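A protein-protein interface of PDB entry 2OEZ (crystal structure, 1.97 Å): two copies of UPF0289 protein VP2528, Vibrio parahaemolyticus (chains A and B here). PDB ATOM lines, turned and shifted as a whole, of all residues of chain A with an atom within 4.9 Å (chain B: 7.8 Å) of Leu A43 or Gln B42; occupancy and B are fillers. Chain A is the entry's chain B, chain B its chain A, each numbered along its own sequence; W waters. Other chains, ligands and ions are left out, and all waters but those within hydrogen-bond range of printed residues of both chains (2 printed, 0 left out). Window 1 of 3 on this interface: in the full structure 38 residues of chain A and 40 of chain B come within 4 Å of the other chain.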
ATOM      1  N   GLN A  28       1.993  18.500  34.963  1.00  0.00           N
ATOM      2  CA  GLN A  28       2.170  18.141  33.548  1.00  0.00           C
ATOM      3  C   GLN A  28       2.345  19.397  32.673  1.00  0.00           C
ATOM      4  O   GLN A  28       3.297  19.497  31.890  1.00  0.00           O
ATOM      5  CB  GLN A  28       0.971  17.351  33.047  1.00  0.00           C
ATOM      6  CG  GLN A  28       1.126  16.912  31.581  1.00  0.00           C
ATOM      7  CD  GLN A  28      -0.003  16.001  31.126  1.00  0.00           C
ATOM      8  OE1 GLN A  28      -0.442  15.094  31.866  1.00  0.00           O
ATOM      9  NE2 GLN A  28      -0.474  16.223  29.899  1.00  0.00           N
ATOM     10  N   ALA A  29       1.477  20.396  32.843  1.00  0.00           N
ATOM     11  CA  ALA A  29       1.695  21.611  32.029  1.00  0.00           C
ATOM     12  C   ALA A  29       3.008  22.276  32.429  1.00  0.00           C
ATOM     13  O   ALA A  29       3.741  22.692  31.570  1.00  0.00           O
ATOM     14  CB  ALA A  29       0.564  22.554  32.118  1.00  0.00           C
ATOM     15  N   ALA A  32       6.153  20.549  30.905  1.00  0.00           N
ATOM     16  CA  ALA A  32       6.152  20.629  29.446  1.00  0.00           C
ATOM     17  C   ALA A  32       6.420  22.087  28.908  1.00  0.00           C
ATOM     18  O   ALA A  32       6.806  22.285  27.758  1.00  0.00           O
ATOM     19  CB  ALA A  32       4.844  20.020  28.890  1.00  0.00           C
ATOM     20  N   HIS A  39       8.269  17.122  21.443  1.00  0.00           N
ATOM     21  CA  HIS A  39       6.931  16.574  21.767  1.00  0.00           C
ATOM     22  C   HIS A  39       6.298  17.037  23.083  1.00  0.00           C
ATOM     23  O   HIS A  39       5.125  16.741  23.352  1.00  0.00           O
ATOM     24  CB  HIS A  39       6.921  15.045  21.676  1.00  0.00           C
ATOM     25  CG  HIS A  39       6.985  14.541  20.272  1.00  0.00           C
ATOM     26  ND1 HIS A  39       8.140  14.039  19.716  1.00  0.00           N
ATOM     27  CD2 HIS A  39       6.048  14.504  19.297  1.00  0.00           C
ATOM     28  CE1 HIS A  39       7.910  13.696  18.461  1.00  0.00           C
ATOM     29  NE2 HIS A  39       6.648  13.971  18.182  1.00  0.00           N
ATOM     30  N   GLN A  40       7.043  17.764  23.905  1.00  0.00           N
ATOM     31  CA  GLN A  40       6.412  18.317  25.092  1.00  0.00           C
ATOM     32  C   GLN A  40       5.160  19.176  24.850  1.00  0.00           C
ATOM     33  O   GLN A  40       4.319  19.279  25.739  1.00  0.00           O
ATOM     34  CB  GLN A  40       7.407  19.181  25.862  1.00  0.00           C
ATOM     35  CG  GLN A  40       8.778  18.594  25.971  1.00  0.00           C
ATOM     36  CD  GLN A  40       9.301  18.660  27.385  1.00  0.00           C
ATOM     37  OE1 GLN A  40       9.464  19.748  27.970  1.00  0.00           O
ATOM     38  NE2 GLN A  40       9.573  17.478  27.959  1.00  0.00           N
ATOM     39  N   TYR A  41       5.065  19.846  23.693  1.00  0.00           N
ATOM     40  CA  TYR A  41       3.927  20.756  23.474  1.00  0.00           C
ATOM     41  C   TYR A  41       2.666  19.911  23.508  1.00  0.00           C
ATOM     42  O   TYR A  41       1.638  20.368  23.948  1.00  0.00           O
ATOM     43  CB  TYR A  41       4.041  21.487  22.112  1.00  0.00           C
ATOM     44  CG  TYR A  41       3.672  20.628  20.959  1.00  0.00           C
ATOM     45  CD1 TYR A  41       4.640  19.937  20.256  1.00  0.00           C
ATOM     46  CD2 TYR A  41       2.345  20.474  20.580  1.00  0.00           C
ATOM     47  CE1 TYR A  41       4.308  19.139  19.174  1.00  0.00           C
ATOM     48  CE2 TYR A  41       1.996  19.661  19.503  1.00  0.00           C
ATOM     49  CZ  TYR A  41       2.977  19.011  18.819  1.00  0.00           C
ATOM     50  OH  TYR A  41       2.639  18.195  17.792  1.00  0.00           O
ATOM     51  N   GLN A  42       2.744  18.660  23.049  1.00  0.00           N
ATOM     52  CA  GLN A  42       1.585  17.753  23.197  1.00  0.00           C
ATOM     53  C   GLN A  42       1.092  17.667  24.652  1.00  0.00           C
ATOM     54  O   GLN A  42      -0.101  17.720  24.896  1.00  0.00           O
ATOM     55  CB  GLN A  42       1.926  16.334  22.769  1.00  0.00           C
ATOM     56  CG  GLN A  42       2.213  16.112  21.267  1.00  0.00           C
ATOM     57  CD  GLN A  42       0.944  16.130  20.417  1.00  0.00           C
ATOM     58  OE1 GLN A  42      -0.149  16.430  20.922  1.00  0.00           O
ATOM     59  NE2 GLN A  42       1.079  15.792  19.118  1.00  0.00           N
ATOM     60  N   LEU A  43       2.004  17.484  25.599  1.00  0.00           N
ATOM     61  CA  LEU A  43       1.612  17.338  27.052  1.00  0.00           C
ATOM     62  C   LEU A  43       1.110  18.667  27.643  1.00  0.00           C
ATOM     63  O   LEU A  43       0.224  18.713  28.546  1.00  0.00           O
ATOM     64  CB  LEU A  43       2.816  16.896  27.874  1.00  0.00           C
ATOM     65  CG  LEU A  43       3.319  15.467  27.583  1.00  0.00           C
ATOM     66  CD1 LEU A  43       4.721  15.240  28.149  1.00  0.00           C
ATOM     67  CD2 LEU A  43       2.350  14.424  28.085  1.00  0.00           C
ATOM     68  N   PHE A  44       1.705  19.755  27.135  1.00  0.00           N
ATOM     69  CA  PHE A  44       1.368  21.076  27.633  1.00  0.00           C
ATOM     70  C   PHE A  44      -0.057  21.441  27.280  1.00  0.00           C
ATOM     71  O   PHE A  44      -0.850  21.785  28.161  1.00  0.00           O
ATOM     72  CB  PHE A  44       2.373  22.165  27.161  1.00  0.00           C
ATOM     73  CG  PHE A  44       1.955  23.527  27.547  1.00  0.00           C
ATOM     74  CD1 PHE A  44       2.186  23.995  28.877  1.00  0.00           C
ATOM     75  CD2 PHE A  44       1.260  24.352  26.637  1.00  0.00           C
ATOM     76  CE1 PHE A  44       1.763  25.241  29.268  1.00  0.00           C
ATOM     77  CE2 PHE A  44       0.842  25.598  27.011  1.00  0.00           C
ATOM     78  CZ  PHE A  44       1.087  26.065  28.353  1.00  0.00           C
ATOM     79  N   PHE A  45      -0.395  21.355  26.003  1.00  0.00           N
ATOM     80  CA  PHE A  45      -1.719  21.787  25.575  1.00  0.00           C
ATOM     81  C   PHE A  45      -2.775  20.743  25.984  1.00  0.00           C
ATOM     82  O   PHE A  45      -3.894  21.103  26.367  1.00  0.00           O
ATOM     83  CB  PHE A  45      -1.795  22.058  24.051  1.00  0.00           C
ATOM     84  CG  PHE A  45      -1.016  23.248  23.611  1.00  0.00           C
ATOM     85  CD1 PHE A  45      -1.503  24.544  23.858  1.00  0.00           C
ATOM     86  CD2 PHE A  45       0.216  23.088  22.951  1.00  0.00           C
ATOM     87  CE1 PHE A  45      -0.771  25.671  23.464  1.00  0.00           C
ATOM     88  CE2 PHE A  45       0.960  24.220  22.530  1.00  0.00           C
ATOM     89  CZ  PHE A  45       0.453  25.524  22.832  1.00  0.00           C
ATOM     90  N   ARG A  46      -2.437  19.456  25.963  1.00  0.00           N
ATOM     91  CA  ARG A  46      -3.445  18.496  26.476  1.00  0.00           C
ATOM     92  C   ARG A  46      -3.840  18.782  27.948  1.00  0.00           C
ATOM     93  O   ARG A  46      -5.033  18.812  28.302  1.00  0.00           O
ATOM     94  CB  ARG A  46      -3.051  17.036  26.202  1.00  0.00           C
ATOM     95  CG  ARG A  46      -4.229  16.047  26.371  1.00  0.00           C
ATOM     96  CD  ARG A  46      -3.937  14.777  25.648  1.00  0.00           C
ATOM     97  NE  ARG A  46      -3.585  15.094  24.271  1.00  0.00           N
ATOM     98  CZ  ARG A  46      -4.262  14.705  23.189  1.00  0.00           C
ATOM     99  NH1 ARG A  46      -5.327  13.909  23.302  1.00  0.00           N
ATOM    100  NH2 ARG A  46      -3.855  15.107  21.992  1.00  0.00           N
ATOM    101  N   ALA A  47      -2.854  19.083  28.775  1.00  0.00           N
ATOM    102  CA  ALA A  47      -3.103  19.467  30.186  1.00  0.00           C
ATOM    103  C   ALA A  47      -3.948  20.725  30.361  1.00  0.00           C
ATOM    104  O   ALA A  47      -4.868  20.763  31.196  1.00  0.00           O
ATOM    105  CB  ALA A  47      -1.769  19.660  30.890  1.00  0.00           C
ATOM    106  N   GLN B  28       6.796   9.862  18.263  1.00  0.00           N
ATOM    107  CA  GLN B  28       6.410  10.210  19.608  1.00  0.00           C
ATOM    108  C   GLN B  28       6.637   9.038  20.576  1.00  0.00           C
ATOM    109  O   GLN B  28       7.135   9.228  21.667  1.00  0.00           O
ATOM    110  CB  GLN B  28       4.932  10.558  19.558  1.00  0.00           C
ATOM    111  CG  GLN B  28       4.340  10.868  20.900  1.00  0.00           C
ATOM    112  CD  GLN B  28       2.908  11.324  20.755  1.00  0.00           C
ATOM    113  OE1 GLN B  28       2.556  12.068  19.799  1.00  0.00           O
ATOM    114  NE2 GLN B  28       2.056  10.876  21.682  1.00  0.00           N
ATOM    115  N   ALA B  32       9.438   9.034  23.579  1.00  0.00           N
ATOM    116  CA  ALA B  32       8.875   8.851  24.876  1.00  0.00           C
ATOM    117  C   ALA B  32       9.314   7.525  25.536  1.00  0.00           C
ATOM    118  O   ALA B  32       9.001   7.306  26.691  1.00  0.00           O
ATOM    119  CB  ALA B  32       7.351   8.926  24.749  1.00  0.00           C
ATOM    120  N   PHE B  35      11.476   6.892  29.010  1.00  0.00           N
ATOM    121  CA  PHE B  35      10.789   7.230  30.265  1.00  0.00           C
ATOM    122  C   PHE B  35      11.707   8.116  31.106  1.00  0.00           C
ATOM    123  O   PHE B  35      11.822   7.951  32.332  1.00  0.00           O
ATOM    124  CB  PHE B  35      10.265   5.967  31.002  1.00  0.00           C
ATOM    125  CG  PHE B  35       9.409   5.105  30.134  1.00  0.00           C
ATOM    126  CD1 PHE B  35       8.057   5.388  29.966  1.00  0.00           C
ATOM    127  CD2 PHE B  35       9.973   4.067  29.399  1.00  0.00           C
ATOM    128  CE1 PHE B  35       7.281   4.625  29.090  1.00  0.00           C
ATOM    129  CE2 PHE B  35       9.203   3.323  28.521  1.00  0.00           C
ATOM    130  CZ  PHE B  35       7.852   3.605  28.374  1.00  0.00           C
ATOM    131  N   ASP B  37      11.609  11.385  31.766  1.00  0.00           N
ATOM    132  CA  ASP B  37      10.852  12.299  32.628  1.00  0.00           C
ATOM    133  C   ASP B  37       9.559  11.602  33.026  1.00  0.00           C
ATOM    134  O   ASP B  37       9.003  10.812  32.237  1.00  0.00           O
ATOM    135  CB  ASP B  37      10.504  13.584  31.864  1.00  0.00           C
ATOM    136  CG  ASP B  37      11.740  14.289  31.287  1.00  0.00           C
ATOM    137  OD1 ASP B  37      11.716  14.654  30.081  1.00  0.00           O
ATOM    138  OD2 ASP B  37      12.731  14.485  32.039  1.00  0.00           O
ATOM    139  N   ASN B  38       9.068  11.863  34.229  1.00  0.00           N
ATOM    140  CA  ASN B  38       7.911  11.114  34.739  1.00  0.00           C
ATOM    141  C   ASN B  38       6.544  11.491  34.115  1.00  0.00           C
ATOM    142  O   ASN B  38       5.493  11.148  34.661  1.00  0.00           O
ATOM    143  CB  ASN B  38       7.886  11.150  36.277  1.00  0.00           C
ATOM    144  CG  ASN B  38       9.035  10.358  36.903  1.00  0.00           C
ATOM    145  OD1 ASN B  38      10.041  10.064  36.249  1.00  0.00           O
ATOM    146  ND2 ASN B  38       8.886  10.011  38.181  1.00  0.00           N
ATOM    147  N   HIS B  39       6.565  12.187  32.974  1.00  0.00           N
ATOM    148  CA  HIS B  39       5.339  12.379  32.158  1.00  0.00           C
ATOM    149  C   HIS B  39       5.404  11.743  30.762  1.00  0.00           C
ATOM    150  O   HIS B  39       4.366  11.505  30.134  1.00  0.00           O
ATOM    151  CB  HIS B  39       4.896  13.867  32.122  1.00  0.00           C
ATOM    152  CG  HIS B  39       4.264  14.334  33.398  1.00  0.00           C
ATOM    153  ND1 HIS B  39       3.004  13.928  33.793  1.00  0.00           N
ATOM    154  CD2 HIS B  39       4.732  15.127  34.394  1.00  0.00           C
ATOM    155  CE1 HIS B  39       2.722  14.456  34.976  1.00  0.00           C
ATOM    156  NE2 HIS B  39       3.759  15.176  35.368  1.00  0.00           N
ATOM    157  N   GLN B  40       6.619  11.460  30.311  1.00  0.00           N
ATOM    158  CA  GLN B  40       6.880  10.867  28.990  1.00  0.00           C
ATOM    159  C   GLN B  40       6.079   9.581  28.679  1.00  0.00           C
ATOM    160  O   GLN B  40       5.825   9.270  27.509  1.00  0.00           O
ATOM    161  CB  GLN B  40       8.396  10.615  28.832  1.00  0.00           C
ATOM    162  CG  GLN B  40       9.266  11.915  28.884  1.00  0.00           C
ATOM    163  CD  GLN B  40       9.352  12.602  27.535  1.00  0.00           C
ATOM    164  OE1 GLN B  40       8.816  12.097  26.562  1.00  0.00           O
ATOM    165  NE2 GLN B  40      10.031  13.745  27.467  1.00  0.00           N
ATOM    166  N   TYR B  41       5.686   8.840  29.719  1.00  0.00           N
ATOM    167  CA  TYR B  41       4.849   7.607  29.563  1.00  0.00           C
ATOM    168  C   TYR B  41       3.462   7.916  28.977  1.00  0.00           C
ATOM    169  O   TYR B  41       2.853   7.127  28.253  1.00  0.00           O
ATOM    170  CB  TYR B  41       4.690   6.840  30.898  1.00  0.00           C
ATOM    171  CG  TYR B  41       3.692   7.467  31.809  1.00  0.00           C
ATOM    172  CD1 TYR B  41       4.088   8.429  32.708  1.00  0.00           C
ATOM    173  CD2 TYR B  41       2.335   7.143  31.724  1.00  0.00           C
ATOM    174  CE1 TYR B  41       3.160   9.028  33.600  1.00  0.00           C
ATOM    175  CE2 TYR B  41       1.399   7.761  32.546  1.00  0.00           C
ATOM    176  CZ  TYR B  41       1.819   8.684  33.492  1.00  0.00           C
ATOM    177  OH  TYR B  41       0.897   9.286  34.302  1.00  0.00           O
ATOM    178  N   GLN B  42       2.995   9.097  29.294  1.00  0.00           N
ATOM    179  CA  GLN B  42       1.733   9.600  28.810  1.00  0.00           C
ATOM    180  C   GLN B  42       1.704   9.751  27.292  1.00  0.00           C
ATOM    181  O   GLN B  42       0.693   9.428  26.663  1.00  0.00           O
ATOM    182  CB  GLN B  42       1.482  10.981  29.368  1.00  0.00           C
ATOM    183  CG  GLN B  42       0.027  11.291  29.409  1.00  0.00           C
ATOM    184  CD  GLN B  42      -0.469  11.337  30.813  1.00  0.00           C
ATOM    185  OE1 GLN B  42      -0.738  10.304  31.431  1.00  0.00           O
ATOM    186  NE2 GLN B  42      -0.606  12.552  31.343  1.00  0.00           N
ATOM    187  N   LEU B  43       2.802  10.277  26.743  1.00  0.00           N
ATOM    188  CA  LEU B  43       2.995  10.392  25.271  1.00  0.00           C
ATOM    189  C   LEU B  43       3.168   9.015  24.679  1.00  0.00           C
ATOM    190  O   LEU B  43       2.628   8.728  23.615  1.00  0.00           O
ATOM    191  CB  LEU B  43       4.261  11.188  24.968  1.00  0.00           C
ATOM    192  CG  LEU B  43       4.194  12.669  24.527  1.00  0.00           C
ATOM    193  CD1 LEU B  43       2.844  13.371  24.677  1.00  0.00           C
ATOM    194  CD2 LEU B  43       5.305  13.416  25.198  1.00  0.00           C
ATOM    195  N   PHE B  44       3.933   8.167  25.377  1.00  0.00           N
ATOM    196  CA  PHE B  44       4.209   6.838  24.881  1.00  0.00           C
ATOM    197  C   PHE B  44       2.945   6.013  24.703  1.00  0.00           C
ATOM    198  O   PHE B  44       2.728   5.420  23.637  1.00  0.00           O
ATOM    199  CB  PHE B  44       5.180   6.073  25.794  1.00  0.00           C
ATOM    200  CG  PHE B  44       5.389   4.676  25.346  1.00  0.00           C
ATOM    201  CD1 PHE B  44       6.193   4.430  24.245  1.00  0.00           C
ATOM    202  CD2 PHE B  44       4.701   3.611  25.954  1.00  0.00           C
ATOM    203  CE1 PHE B  44       6.368   3.114  23.773  1.00  0.00           C
ATOM    204  CE2 PHE B  44       4.860   2.314  25.490  1.00  0.00           C
ATOM    205  CZ  PHE B  44       5.681   2.060  24.419  1.00  0.00           C
ATOM    206  N   PHE B  45       2.160   5.884  25.755  1.00  0.00           N
ATOM    207  CA  PHE B  45       0.951   5.031  25.669  1.00  0.00           C
ATOM    208  C   PHE B  45      -0.093   5.630  24.729  1.00  0.00           C
ATOM    209  O   PHE B  45      -0.711   4.891  23.928  1.00  0.00           O
ATOM    210  CB  PHE B  45       0.364   4.734  27.056  1.00  0.00           C
ATOM    211  CG  PHE B  45       1.215   3.761  27.866  1.00  0.00           C
ATOM    212  CD1 PHE B  45       1.327   2.434  27.458  1.00  0.00           C
ATOM    213  CD2 PHE B  45       1.948   4.207  28.977  1.00  0.00           C
ATOM    214  CE1 PHE B  45       2.132   1.521  28.151  1.00  0.00           C
ATOM    215  CE2 PHE B  45       2.797   3.303  29.680  1.00  0.00           C
ATOM    216  CZ  PHE B  45       2.882   1.950  29.252  1.00  0.00           C
ATOM    217  N   ARG B  46      -0.285   6.944  24.800  1.00  0.00           N
ATOM    218  CA  ARG B  46      -1.246   7.578  23.882  1.00  0.00           C
ATOM    219  C   ARG B  46      -0.868   7.398  22.402  1.00  0.00           C
ATOM    220  O   ARG B  46      -1.726   7.120  21.577  1.00  0.00           O
ATOM    221  CB  ARG B  46      -1.500   9.027  24.245  1.00  0.00           C
ATOM    222  CG  ARG B  46      -2.894   9.508  23.809  1.00  0.00           C
ATOM    223  CD  ARG B  46      -2.863  10.243  22.486  1.00  0.00           C
ATOM    224  NE  ARG B  46      -1.960  11.392  22.543  1.00  0.00           N
ATOM    225  CZ  ARG B  46      -1.015  11.676  21.649  1.00  0.00           C
ATOM    226  NH1 ARG B  46      -0.842  10.914  20.561  1.00  0.00           N
ATOM    227  NH2 ARG B  46      -0.256  12.749  21.849  1.00  0.00           N
ATOM    228  N   ALA B  47       0.416   7.493  22.075  1.00  0.00           N
ATOM    229  CA  ALA B  47       0.880   7.117  20.717  1.00  0.00           C
ATOM    230  C   ALA B  47       0.533   5.687  20.316  1.00  0.00           C
ATOM    231  O   ALA B  47       0.054   5.420  19.200  1.00  0.00           O
ATOM    232  CB  ALA B  47       2.392   7.359  20.559  1.00  0.00           C
ATOM    233  N   LEU B  48       0.809   4.747  21.228  1.00  0.00           N
ATOM    234  CA  LEU B  48       0.559   3.360  20.974  1.00  0.00           C
ATOM    235  C   LEU B  48      -0.900   3.135  20.703  1.00  0.00           C
ATOM    236  O   LEU B  48      -1.241   2.431  19.779  1.00  0.00           O
ATOM    237  CB  LEU B  48       1.008   2.524  22.211  1.00  0.00           C
ATOM    238  CG  LEU B  48       1.887   1.322  22.028  1.00  0.00           C
ATOM    239  CD1 LEU B  48       3.147   1.616  21.156  1.00  0.00           C
ATOM    240  CD2 LEU B  48       2.275   0.679  23.443  1.00  0.00           C
ATOM    241  N   PHE B  49      -1.752   3.697  21.548  1.00  0.00           N
ATOM    242  CA  PHE B  49      -3.196   3.468  21.456  1.00  0.00           C
ATOM    243  C   PHE B  49      -3.855   4.198  20.248  1.00  0.00           C
ATOM    244  O   PHE B  49      -4.748   3.649  19.611  1.00  0.00           O
ATOM    245  CB  PHE B  49      -3.891   3.814  22.794  1.00  0.00           C
ATOM    246  CG  PHE B  49      -3.555   2.823  23.938  1.00  0.00           C
ATOM    247  CD1 PHE B  49      -3.471   1.450  23.672  1.00  0.00           C
ATOM    248  CD2 PHE B  49      -3.347   3.281  25.248  1.00  0.00           C
ATOM    249  CE1 PHE B  49      -3.161   0.539  24.677  1.00  0.00           C
ATOM    250  CE2 PHE B  49      -3.032   2.377  26.269  1.00  0.00           C
ATOM    251  CZ  PHE B  49      -2.949   0.999  25.977  1.00  0.00           C
ATOM    252  N   PHE B 126      -7.582   4.171  29.427  1.00  0.00           N
ATOM    253  CA  PHE B 126      -6.532   5.151  29.180  1.00  0.00           C
ATOM    254  C   PHE B 126      -7.108   6.204  28.237  1.00  0.00           C
ATOM    255  O   PHE B 126      -6.797   7.401  28.342  1.00  0.00           O
ATOM    256  CB  PHE B 126      -5.262   4.502  28.595  1.00  0.00           C
ATOM    257  CG  PHE B 126      -4.066   5.415  28.583  1.00  0.00           C
ATOM    258  CD1 PHE B 126      -3.272   5.553  29.714  1.00  0.00           C
ATOM    259  CD2 PHE B 126      -3.748   6.157  27.441  1.00  0.00           C
ATOM    260  CE1 PHE B 126      -2.166   6.412  29.719  1.00  0.00           C
ATOM    261  CE2 PHE B 126      -2.661   7.020  27.441  1.00  0.00           C
ATOM    262  CZ  PHE B 126      -1.863   7.153  28.582  1.00  0.00           C
ATOM    263  N   CYS B 133      -3.550  11.172  35.448  1.00  0.00           N
ATOM    264  CA  CYS B 133      -2.843  10.381  36.477  1.00  0.00           C
ATOM    265  C   CYS B 133      -3.530   9.065  36.841  1.00  0.00           C
ATOM    266  O   CYS B 133      -4.666   8.795  36.428  1.00  0.00           O
ATOM    267  CB  CYS B 133      -2.478  11.211  37.731  1.00  0.00           C
ATOM    268  SG  CYS B 133      -3.733  11.480  39.097  1.00  0.00           S
ATOM    269  N   CYS B 134      -2.835   8.241  37.616  1.00  0.00           N
ATOM    270  CA  CYS B 134      -3.141   6.819  37.618  1.00  0.00           C
ATOM    271  C   CYS B 134      -3.900   6.233  38.796  1.00  0.00           C
ATOM    272  O   CYS B 134      -3.896   5.017  38.974  1.00  0.00           O
ATOM    273  CB  CYS B 134      -1.875   6.008  37.318  1.00  0.00           C
ATOM    274  SG  CYS B 134      -1.175   6.503  35.737  1.00  0.00           S
ATOM    275  N   LEU B 140      -1.320   0.410  35.703  1.00  0.00           N
ATOM    276  CA  LEU B 140      -0.344   1.298  35.078  1.00  0.00           C
ATOM    277  C   LEU B 140       0.566   1.917  36.150  1.00  0.00           C
ATOM    278  O   LEU B 140       1.790   1.954  36.013  1.00  0.00           O
ATOM    279  CB  LEU B 140      -1.023   2.371  34.194  1.00  0.00           C
ATOM    280  CG  LEU B 140      -0.156   3.419  33.510  1.00  0.00           C
ATOM    281  CD1 LEU B 140       0.913   2.717  32.596  1.00  0.00           C
ATOM    282  CD2 LEU B 140      -1.078   4.288  32.579  1.00  0.00           C
ATOM    283  N   LEU B 144       4.588   1.737  36.235  1.00  0.00           N
ATOM    284  CA  LEU B 144       5.484   2.881  36.243  1.00  0.00           C
ATOM    285  C   LEU B 144       6.533   2.801  37.344  1.00  0.00           C
ATOM    286  O   LEU B 144       7.584   3.432  37.254  1.00  0.00           O
ATOM    287  CB  LEU B 144       4.679   4.169  36.356  1.00  0.00           C
ATOM    288  CG  LEU B 144       3.880   4.513  35.100  1.00  0.00           C
ATOM    289  CD1 LEU B 144       2.928   5.653  35.581  1.00  0.00           C
ATOM    290  CD2 LEU B 144       4.822   4.940  34.005  1.00  0.00           C
HETATM  291  O   HOH W   1       8.287  15.244  26.137  1.00  0.00           O
HETATM  292  O   HOH W   2      -1.575  14.128  29.048  1.00  0.00           O
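Water W2 bridges NE2 of Gln A28 (2.5 Å) and NE2 of Gln B42 (2.9 Å).
Water W1 lies within hydrogen-bond range of the side-chain amide nitrogen (NE2) of Gln B40 and the side-chain amide nitrogen (NE2) of Gln A40.
Among the printed residues, pairs that only touch across the chains: Gln A28 with His B39, His A39 with Gln B28, His A39 with Leu B43, Gln A40 with Gln B40, Gln A42 with Leu B43, Gln A42 with Arg B46, Leu A43 with Gln B42 and Leu A43 with Leu B43.
Leu A43 touches just these residues of chain B: Gln B42 and Leu B43.
Gln B42 touches just these residues of chain A: Gln A28 (2.6 Å) and Leu A43 (3.8 Å).
Printed residues of chain A within 4 Å of Arg B46: Gln A42 (3.8 Å).
Printed residues of chain B within 4 Å of Gln A40: Gln B40 (3.8 Å).
Of the printed residues of chain B, Gln A28 touches His B39 (3.8 Å) and Gln B42 (2.6 Å).
Of the printed residues of chain A, Leu B43 touches His A39, Gln A42 and Leu A43.
The nearest printed residue of chain B that does not touch His A39 is Gln B40 (6.0 Å).
The side-chain amide oxygen (OE1) of Gln B42 lies within hydrogen-bond range of the side-chain hydroxyl (OH) of Tyr B41.
The side-chain carboxylate of Asp B37 sits at hydrogen-bond distance from the side-chain amide nitrogen of Gln B40.
The backbone carbonyl oxygen of Leu B43 lies within hydrogen-bond range of the side-chain amide nitrogen of Gln B28 (2.9 Å).
The side-chain amide nitrogen (NE2) of Gln A42 lies within hydrogen-bond range of the side-chain hydroxyl (OH) of Tyr A41, at 3.2 Å.
NE2 of Gln A28 is in hydrogen-bond range of O of Leu A43 (2.9 Å).
NE2 of Gln B28 lies close to NH2 of Arg B46, at 3.0 Å.
Printed residues of chain A that touch a printed residue of chain B: Gln A28, His A39, Gln A40, Gln A42 and Leu A43.
Hydrophobic or aromatic side chains of chain A that line the printed part of chain B: His A39 and Leu A43.
OE1 of Gln A28 sits at hydrogen-bond distance from NE2 of Gln B42 (2.6 Å).
His A39 touches Leu B43, but with the chains exchanged Leu A43 does not touch His B39 (4.1 Å).
Gln B40 touches its own counterpart, Gln A40.
Gln A42 touches Leu B43, and with the chains exchanged Leu A43 touches Gln B42.
Gln A42 touches Arg B46, but with the chains exchanged Arg A46 does not touch Gln B42 (6.5 Å).
Of the 9 pairs that touch across the chains among the printed residues, 6 have their exchanged pair printed and touching as well.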
